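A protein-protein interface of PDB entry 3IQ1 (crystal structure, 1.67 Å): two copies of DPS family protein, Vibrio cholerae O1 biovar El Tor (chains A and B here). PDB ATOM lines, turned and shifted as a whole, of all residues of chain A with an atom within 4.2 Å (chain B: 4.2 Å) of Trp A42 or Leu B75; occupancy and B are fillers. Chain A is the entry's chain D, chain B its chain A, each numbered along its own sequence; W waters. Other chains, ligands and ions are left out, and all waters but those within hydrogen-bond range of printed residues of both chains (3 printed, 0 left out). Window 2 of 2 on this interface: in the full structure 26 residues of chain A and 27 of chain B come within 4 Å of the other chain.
The backbone carbonyl oxygen of Glu B72 is in hydrogen-bond range of the side-chain hydroxyl of Thr B76 (2.8 Å). O of Pro B81 is in hydrogen-bond range of ND1 of His B83, at 2.8 Å. The side-chain amide nitrogen (NE2) of Gln B31 lies within hydrogen-bond range of the side-chain hydroxyl (OH) of Tyr B88 (3.1 Å). O of Met B82 lies within hydrogen-bond range of OH of Tyr B88 (2.7 Å). The backbone carbonyl oxygen of Gly A39 lies close to the side-chain amide oxygen of Asn A43 (3.2 Å).
Printed residues of chain A that touch a printed residue of chain B: Met A35, Arg A38, His A41, Trp A42 and Asn A43. Hydrophobic or aromatic side chains of chain A within 4 Å of the printed part of chain B: Met A35, His A41 and Trp A42. Printed residues of chain B that touch a printed residue of chain A: Ile B67, Ala B71, Glu B72, Leu B75, Pro B81, Met B82, His B83 and Tyr B88.
Among the printed residues, merely in contact across the chains: Trp A42 with Ala B71 (3.2 Å), Trp A42 with Leu B75 (3.3 Å), Arg A38 with Ile B67 (3.4 Å), Met A35 with Tyr B88 (3.7 Å), Met A35 with His B83 (3.7 Å), Trp A42 with Tyr B88 (3.7 Å), His A41 with Glu B72 (3.8 Å), Trp A42 with His B83 (3.8 Å), Trp A42 with Met B82 (3.9 Å), Asn A43 with Pro B81 (3.9 Å) and Asn A43 with Leu B75 (3.9 Å).
Printed residues of chain B within 4 Å of Trp A42: Ala B71, Leu B75, Met B82, His B83 and Tyr B88. Printed residues of chain A within 4 Å of Leu B75: Trp A42 and Asn A43. Of the printed residues of chain A, Tyr B88 touches Met A35 (3.7 Å) and Trp A42 (3.7 Å). Printed residues of chain B within 4 Å of His A41: Glu B72. Of the printed residues of chain A, Met B82 touches Trp A42 (3.9 Å). Of the printed residues of chain B, Asn A43 touches Leu B75 (3.9 Å), Pro B81 (3.9 Å) and His B83 (3.2 Å). The nearest printed residue of chain B that does not touch Trp A42 is Gln B31 (4.02 Å). The nearest printed residue of chain A that does not touch Leu B75 is His A41 (6.0 Å). The nearest printed residue of chain A that does not touch Ile B67 is Trp A42 (4.02 Å).
NE2 of His B83 lies within hydrogen-bond range of OD1 of Asn A43 (3.2 Å).
Water W2 lies within hydrogen-bond range of OE2 of Glu B72 (2.6 Å) and NE2 of His A41 (3.5 Å). Water W1 lies within hydrogen-bond range of NE1 of Trp A42 (2.7 Å) and OE2 of Glu B72 (3.4 Å). Water W3 bridges NE2 of Gln B31 and NE of Arg A38.
No position is printed for both chains.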
ATOM      1  N   MET A  35     -13.698 -29.778  23.516  1.00  0.00           N
ATOM      2  CA  MET A  35     -12.282 -29.589  23.140  1.00  0.00           C
ATOM      3  C   MET A  35     -12.025 -30.240  21.802  1.00  0.00           C
ATOM      4  O   MET A  35     -11.399 -29.640  20.947  1.00  0.00           O
ATOM      5  CB  MET A  35     -11.376 -30.236  24.178  1.00  0.00           C
ATOM      6  CG  MET A  35      -9.913 -29.914  24.046  1.00  0.00           C
ATOM      7  SD  MET A  35      -9.547 -27.956  24.201  1.00  0.00           S
ATOM      8  CE  MET A  35      -9.364 -27.528  22.511  1.00  0.00           C
ATOM      9  N   ARG A  38     -13.545 -28.059  19.099  1.00  0.00           N
ATOM     10  CA  ARG A  38     -12.680 -26.916  18.862  1.00  0.00           C
ATOM     11  C   ARG A  38     -11.544 -27.277  17.942  1.00  0.00           C
ATOM     12  O   ARG A  38     -11.200 -26.528  17.019  1.00  0.00           O
ATOM     13  CB  ARG A  38     -12.118 -26.357  20.174  1.00  0.00           C
ATOM     14  CG  ARG A  38     -13.119 -25.590  20.934  1.00  0.00           C
ATOM     15  CD  ARG A  38     -13.086 -24.218  20.421  1.00  0.00           C
ATOM     16  NE  ARG A  38     -12.421 -23.335  21.374  1.00  0.00           N
ATOM     17  CZ  ARG A  38     -12.311 -22.054  21.188  1.00  0.00           C
ATOM     18  NH1 ARG A  38     -12.806 -21.545  20.082  1.00  0.00           N
ATOM     19  NH2 ARG A  38     -11.759 -21.267  22.116  1.00  0.00           N
ATOM     20  N   GLY A  39     -10.938 -28.420  18.196  1.00  0.00           N
ATOM     21  CA  GLY A  39      -9.950 -28.979  17.317  1.00  0.00           C
ATOM     22  C   GLY A  39     -10.448 -29.221  15.883  1.00  0.00           C
ATOM     23  O   GLY A  39      -9.767 -28.934  14.909  1.00  0.00           O
ATOM     24  N   TYR A  40     -11.634 -29.787  15.743  1.00  0.00           N
ATOM     25  CA  TYR A  40     -12.200 -29.986  14.413  1.00  0.00           C
ATOM     26  C   TYR A  40     -12.294 -28.643  13.680  1.00  0.00           C
ATOM     27  O   TYR A  40     -12.028 -28.547  12.458  1.00  0.00           O
ATOM     28  CB  TYR A  40     -13.607 -30.644  14.494  1.00  0.00           C
ATOM     29  CG  TYR A  40     -13.718 -31.983  15.197  1.00  0.00           C
ATOM     30  CD1 TYR A  40     -12.638 -32.816  15.356  1.00  0.00           C
ATOM     31  CD2 TYR A  40     -14.948 -32.409  15.670  1.00  0.00           C
ATOM     32  CE1 TYR A  40     -12.761 -34.043  15.999  1.00  0.00           C
ATOM     33  CE2 TYR A  40     -15.114 -33.608  16.258  1.00  0.00           C
ATOM     34  CZ  TYR A  40     -14.035 -34.427  16.447  1.00  0.00           C
ATOM     35  OH  TYR A  40     -14.222 -35.631  17.061  1.00  0.00           O
ATOM     36  N   HIS A  41     -12.706 -27.584  14.388  1.00  0.00           N
ATOM     37  CA  HIS A  41     -12.855 -26.209  13.842  1.00  0.00           C
ATOM     38  C   HIS A  41     -11.513 -25.689  13.361  1.00  0.00           C
ATOM     39  O   HIS A  41     -11.397 -25.150  12.272  1.00  0.00           O
ATOM     40  CB  HIS A  41     -13.451 -25.314  14.914  1.00  0.00           C
ATOM     41  CG  HIS A  41     -13.448 -23.845  14.606  1.00  0.00           C
ATOM     42  ND1 HIS A  41     -12.712 -22.929  15.321  1.00  0.00           N
ATOM     43  CD2 HIS A  41     -14.140 -23.140  13.675  1.00  0.00           C
ATOM     44  CE1 HIS A  41     -12.943 -21.714  14.822  1.00  0.00           C
ATOM     45  NE2 HIS A  41     -13.810 -21.830  13.824  1.00  0.00           N
ATOM     46  N   TRP A  42     -10.513 -25.817  14.213  1.00  0.00           N
ATOM     47  CA  TRP A  42      -9.204 -25.271  13.921  1.00  0.00           C
ATOM     48  C   TRP A  42      -8.513 -26.024  12.785  1.00  0.00           C
ATOM     49  O   TRP A  42      -7.858 -25.404  11.929  1.00  0.00           O
ATOM     50  CB  TRP A  42      -8.293 -25.305  15.156  1.00  0.00           C
ATOM     51  CG  TRP A  42      -8.641 -24.322  16.206  1.00  0.00           C
ATOM     52  CD1 TRP A  42      -9.286 -23.103  16.039  1.00  0.00           C
ATOM     53  CD2 TRP A  42      -8.404 -24.456  17.601  1.00  0.00           C
ATOM     54  NE1 TRP A  42      -9.478 -22.514  17.254  1.00  0.00           N
ATOM     55  CE2 TRP A  42      -8.941 -23.313  18.230  1.00  0.00           C
ATOM     56  CE3 TRP A  42      -7.828 -25.443  18.386  1.00  0.00           C
ATOM     57  CZ2 TRP A  42      -8.849 -23.112  19.587  1.00  0.00           C
ATOM     58  CZ3 TRP A  42      -7.764 -25.263  19.765  1.00  0.00           C
ATOM     59  CH2 TRP A  42      -8.283 -24.098  20.349  1.00  0.00           C
ATOM     60  N   ASN A  43      -8.675 -27.343  12.759  1.00  0.00           N
ATOM     61  CA  ASN A  43      -7.830 -28.201  11.912  1.00  0.00           C
ATOM     62  C   ASN A  43      -8.403 -28.644  10.545  1.00  0.00           C
ATOM     63  O   ASN A  43      -7.738 -29.293   9.774  1.00  0.00           O
ATOM     64  CB  ASN A  43      -7.394 -29.426  12.718  1.00  0.00           C
ATOM     65  CG  ASN A  43      -6.532 -29.053  13.962  1.00  0.00           C
ATOM     66  OD1 ASN A  43      -6.669 -29.676  15.044  1.00  0.00           O
ATOM     67  ND2 ASN A  43      -5.673 -28.039  13.813  1.00  0.00           N
ATOM     68  N   ILE A  44      -9.658 -28.321  10.290  1.00  0.00           N
ATOM     69  CA  ILE A  44     -10.262 -28.673   9.002  1.00  0.00           C
ATOM     70  C   ILE A  44      -9.444 -28.092   7.846  1.00  0.00           C
ATOM     71  O   ILE A  44      -8.959 -26.972   7.921  1.00  0.00           O
ATOM     72  CB  ILE A  44     -11.741 -28.221   8.982  1.00  0.00           C
ATOM     73  CG1 ILE A  44     -12.448 -28.706   7.727  1.00  0.00           C
ATOM     74  CG2 ILE A  44     -11.906 -26.703   9.114  1.00  0.00           C
ATOM     75  CD1 ILE A  44     -12.584 -30.235   7.626  1.00  0.00           C
ATOM     76  N   GLN B  31      -5.450 -21.650  28.255  1.00  0.00           N
ATOM     77  CA  GLN B  31      -6.489 -22.666  28.389  1.00  0.00           C
ATOM     78  C   GLN B  31      -6.677 -23.072  29.870  1.00  0.00           C
ATOM     79  O   GLN B  31      -7.809 -23.067  30.387  1.00  0.00           O
ATOM     80  CB  GLN B  31      -6.146 -23.873  27.509  1.00  0.00           C
ATOM     81  CG  GLN B  31      -6.355 -23.650  26.016  1.00  0.00           C
ATOM     82  CD  GLN B  31      -7.806 -23.797  25.592  1.00  0.00           C
ATOM     83  OE1 GLN B  31      -8.693 -23.521  26.380  1.00  0.00           O
ATOM     84  NE2 GLN B  31      -8.058 -24.214  24.359  1.00  0.00           N
ATOM     85  N   ILE B  67      -8.023 -17.091  22.923  1.00  0.00           N
ATOM     86  CA  ILE B  67      -7.688 -18.470  22.626  1.00  0.00           C
ATOM     87  C   ILE B  67      -7.902 -18.792  21.125  1.00  0.00           C
ATOM     88  O   ILE B  67      -7.018 -19.432  20.455  1.00  0.00           O
ATOM     89  CB  ILE B  67      -8.433 -19.439  23.526  1.00  0.00           C
ATOM     90  CG1 ILE B  67      -7.841 -19.396  24.949  1.00  0.00           C
ATOM     91  CG2 ILE B  67      -8.442 -20.857  22.892  1.00  0.00           C
ATOM     92  CD1 ILE B  67      -8.747 -19.997  26.039  1.00  0.00           C
ATOM     93  N   ALA B  71      -4.865 -19.730  18.449  1.00  0.00           N
ATOM     94  CA  ALA B  71      -4.816 -20.951  17.711  1.00  0.00           C
ATOM     95  C   ALA B  71      -4.714 -20.634  16.223  1.00  0.00           C
ATOM     96  O   ALA B  71      -3.981 -21.305  15.474  1.00  0.00           O
ATOM     97  CB  ALA B  71      -6.075 -21.803  17.988  1.00  0.00           C
ATOM     98  N   GLU B  72      -5.444 -19.611  15.803  1.00  0.00           N
ATOM     99  CA  GLU B  72      -5.481 -19.240  14.388  1.00  0.00           C
ATOM    100  C   GLU B  72      -4.182 -18.624  13.959  1.00  0.00           C
ATOM    101  O   GLU B  72      -3.789 -18.854  12.854  1.00  0.00           O
ATOM    102  CB  GLU B  72      -6.675 -18.376  14.035  1.00  0.00           C
ATOM    103  CG  GLU B  72      -7.881 -19.317  14.055  1.00  0.00           C
ATOM    104  CD  GLU B  72      -9.156 -18.733  13.549  1.00  0.00           C
ATOM    105  OE1 GLU B  72      -9.205 -17.518  13.279  1.00  0.00           O
ATOM    106  OE2 GLU B  72     -10.133 -19.533  13.486  1.00  0.00           O
ATOM    107  N   ARG B  73      -3.502 -17.916  14.853  1.00  0.00           N
ATOM    108  CA  ARG B  73      -2.187 -17.364  14.518  1.00  0.00           C
ATOM    109  C   ARG B  73      -1.178 -18.495  14.341  1.00  0.00           C
ATOM    110  O   ARG B  73      -0.366 -18.475  13.427  1.00  0.00           O
ATOM    111  CB  ARG B  73      -1.705 -16.375  15.579  1.00  0.00           C
ATOM    112  CG  ARG B  73      -0.405 -15.650  15.183  1.00  0.00           C
ATOM    113  CD  ARG B  73      -0.591 -14.672  14.057  1.00  0.00           C
ATOM    114  NE  ARG B  73       0.689 -14.277  13.474  1.00  0.00           N
ATOM    115  CZ  ARG B  73       0.793 -13.688  12.283  1.00  0.00           C
ATOM    116  NH1 ARG B  73      -0.300 -13.402  11.582  1.00  0.00           N
ATOM    117  NH2 ARG B  73       2.017 -13.473  11.778  1.00  0.00           N
ATOM    118  N   ILE B  74      -1.267 -19.530  15.201  1.00  0.00           N
ATOM    119  CA  ILE B  74      -0.403 -20.688  15.078  1.00  0.00           C
ATOM    120  C   ILE B  74      -0.589 -21.367  13.722  1.00  0.00           C
ATOM    121  O   ILE B  74       0.396 -21.740  13.075  1.00  0.00           O
ATOM    122  CB  ILE B  74      -0.577 -21.654  16.310  1.00  0.00           C
ATOM    123  CG1 ILE B  74      -0.162 -20.918  17.592  1.00  0.00           C
ATOM    124  CG2 ILE B  74       0.085 -23.008  16.042  1.00  0.00           C
ATOM    125  CD1 ILE B  74      -0.755 -21.528  18.902  1.00  0.00           C
ATOM    126  N   LEU B  75      -1.851 -21.580  13.335  1.00  0.00           N
ATOM    127  CA  LEU B  75      -2.215 -22.139  12.059  1.00  0.00           C
ATOM    128  C   LEU B  75      -1.710 -21.273  10.902  1.00  0.00           C
ATOM    129  O   LEU B  75      -1.238 -21.803   9.884  1.00  0.00           O
ATOM    130  CB  LEU B  75      -3.715 -22.282  11.970  1.00  0.00           C
ATOM    131  CG  LEU B  75      -4.294 -23.423  12.812  1.00  0.00           C
ATOM    132  CD1 LEU B  75      -5.799 -23.141  13.071  1.00  0.00           C
ATOM    133  CD2 LEU B  75      -4.079 -24.816  12.178  1.00  0.00           C
ATOM    134  N   THR B  76      -1.768 -19.977  11.088  1.00  0.00           N
ATOM    135  CA  THR B  76      -1.350 -19.001  10.083  1.00  0.00           C
ATOM    136  C   THR B  76       0.146 -19.099   9.845  1.00  0.00           C
ATOM    137  O   THR B  76       0.616 -18.851   8.701  1.00  0.00           O
ATOM    138  CB  THR B  76      -1.812 -17.571  10.491  1.00  0.00           C
ATOM    139  OG1 THR B  76      -3.251 -17.508  10.454  1.00  0.00           O
ATOM    140  CG2 THR B  76      -1.275 -16.448   9.577  1.00  0.00           C
ATOM    141  N   LEU B  77       0.887 -19.482  10.891  1.00  0.00           N
ATOM    142  CA  LEU B  77       2.344 -19.677  10.810  1.00  0.00           C
ATOM    143  C   LEU B  77       2.699 -21.087  10.302  1.00  0.00           C
ATOM    144  O   LEU B  77       3.839 -21.501  10.386  1.00  0.00           O
ATOM    145  CB  LEU B  77       2.998 -19.442  12.168  1.00  0.00           C
ATOM    146  CG  LEU B  77       2.999 -17.984  12.655  1.00  0.00           C
ATOM    147  CD1 LEU B  77       3.442 -17.929  14.103  1.00  0.00           C
ATOM    148  CD2 LEU B  77       3.892 -17.080  11.775  1.00  0.00           C
ATOM    149  N   SER B  78       1.719 -21.823   9.801  1.00  0.00           N
ATOM    150  CA  SER B  78       1.882 -23.180   9.305  1.00  0.00           C
ATOM    151  C   SER B  78       2.306 -24.151  10.402  1.00  0.00           C
ATOM    152  O   SER B  78       3.147 -25.020  10.175  1.00  0.00           O
ATOM    153  CB  SER B  78       2.868 -23.208   8.135  1.00  0.00           C
ATOM    154  OG  SER B  78       2.329 -22.477   7.029  1.00  0.00           O
ATOM    155  N   ALA B  79       1.769 -23.973  11.611  1.00  0.00           N
ATOM    156  CA  ALA B  79       2.072 -24.874  12.698  1.00  0.00           C
ATOM    157  C   ALA B  79       0.780 -25.449  13.252  1.00  0.00           C
ATOM    158  O   ALA B  79      -0.308 -25.080  12.823  1.00  0.00           O
ATOM    159  CB  ALA B  79       2.893 -24.136  13.786  1.00  0.00           C
ATOM    160  N   PRO B  81      -1.707 -26.043  16.301  1.00  0.00           N
ATOM    161  CA  PRO B  81      -2.075 -25.579  17.615  1.00  0.00           C
ATOM    162  C   PRO B  81      -2.362 -26.779  18.518  1.00  0.00           C
ATOM    163  O   PRO B  81      -3.075 -27.695  18.112  1.00  0.00           O
ATOM    164  CB  PRO B  81      -3.357 -24.767  17.365  1.00  0.00           C
ATOM    165  CG  PRO B  81      -3.921 -25.329  16.120  1.00  0.00           C
ATOM    166  CD  PRO B  81      -2.784 -25.878  15.316  1.00  0.00           C
ATOM    167  N   MET B  82      -1.847 -26.748  19.729  1.00  0.00           N
ATOM    168  CA  MET B  82      -2.209 -27.757  20.708  1.00  0.00           C
ATOM    169  C   MET B  82      -3.736 -27.680  20.899  1.00  0.00           C
ATOM    170  O   MET B  82      -4.311 -26.602  20.927  1.00  0.00           O
ATOM    171  CB  MET B  82      -1.473 -27.509  22.030  1.00  0.00           C
ATOM    172  CG  MET B  82      -0.272 -28.334  22.209  1.00  0.00           C
ATOM    173  SD  MET B  82       0.386 -28.007  24.049  1.00  0.00           S
ATOM    174  CE  MET B  82       0.970 -26.305  23.763  1.00  0.00           C
ATOM    175  N   HIS B  83      -4.361 -28.836  21.053  1.00  0.00           N
ATOM    176  CA  HIS B  83      -5.828 -28.924  21.062  1.00  0.00           C
ATOM    177  C   HIS B  83      -6.340 -30.117  21.879  1.00  0.00           C
ATOM    178  O   HIS B  83      -7.353 -30.745  21.541  1.00  0.00           O
ATOM    179  CB  HIS B  83      -6.452 -28.859  19.652  1.00  0.00           C
ATOM    180  CG  HIS B  83      -5.991 -29.945  18.714  1.00  0.00           C
ATOM    181  ND1 HIS B  83      -4.747 -29.927  18.112  1.00  0.00           N
ATOM    182  CD2 HIS B  83      -6.625 -31.051  18.253  1.00  0.00           C
ATOM    183  CE1 HIS B  83      -4.645 -30.962  17.290  1.00  0.00           C
ATOM    184  NE2 HIS B  83      -5.767 -31.671  17.366  1.00  0.00           N
ATOM    185  N   TYR B  88      -2.255 -29.415  26.949  1.00  0.00           N
ATOM    186  CA  TYR B  88      -2.183 -28.180  27.715  1.00  0.00           C
ATOM    187  C   TYR B  88      -1.604 -28.362  29.116  1.00  0.00           C
ATOM    188  O   TYR B  88      -0.841 -27.529  29.585  1.00  0.00           O
ATOM    189  CB  TYR B  88      -3.558 -27.504  27.842  1.00  0.00           C
ATOM    190  CG  TYR B  88      -4.222 -27.130  26.538  1.00  0.00           C
ATOM    191  CD1 TYR B  88      -3.485 -26.607  25.504  1.00  0.00           C
ATOM    192  CD2 TYR B  88      -5.574 -27.296  26.363  1.00  0.00           C
ATOM    193  CE1 TYR B  88      -4.060 -26.230  24.300  1.00  0.00           C
ATOM    194  CE2 TYR B  88      -6.177 -26.923  25.151  1.00  0.00           C
ATOM    195  CZ  TYR B  88      -5.404 -26.409  24.125  1.00  0.00           C
ATOM    196  OH  TYR B  88      -6.036 -26.035  22.962  1.00  0.00           O
HETATM  197  O   HOH W   1     -10.672 -20.073  16.832  1.00  0.00           O
HETATM  198  O   HOH W   2     -12.191 -18.972  14.951  1.00  0.00           O
HETATM  199  O   HOH W   3     -10.993 -24.459  23.800  1.00  0.00           O
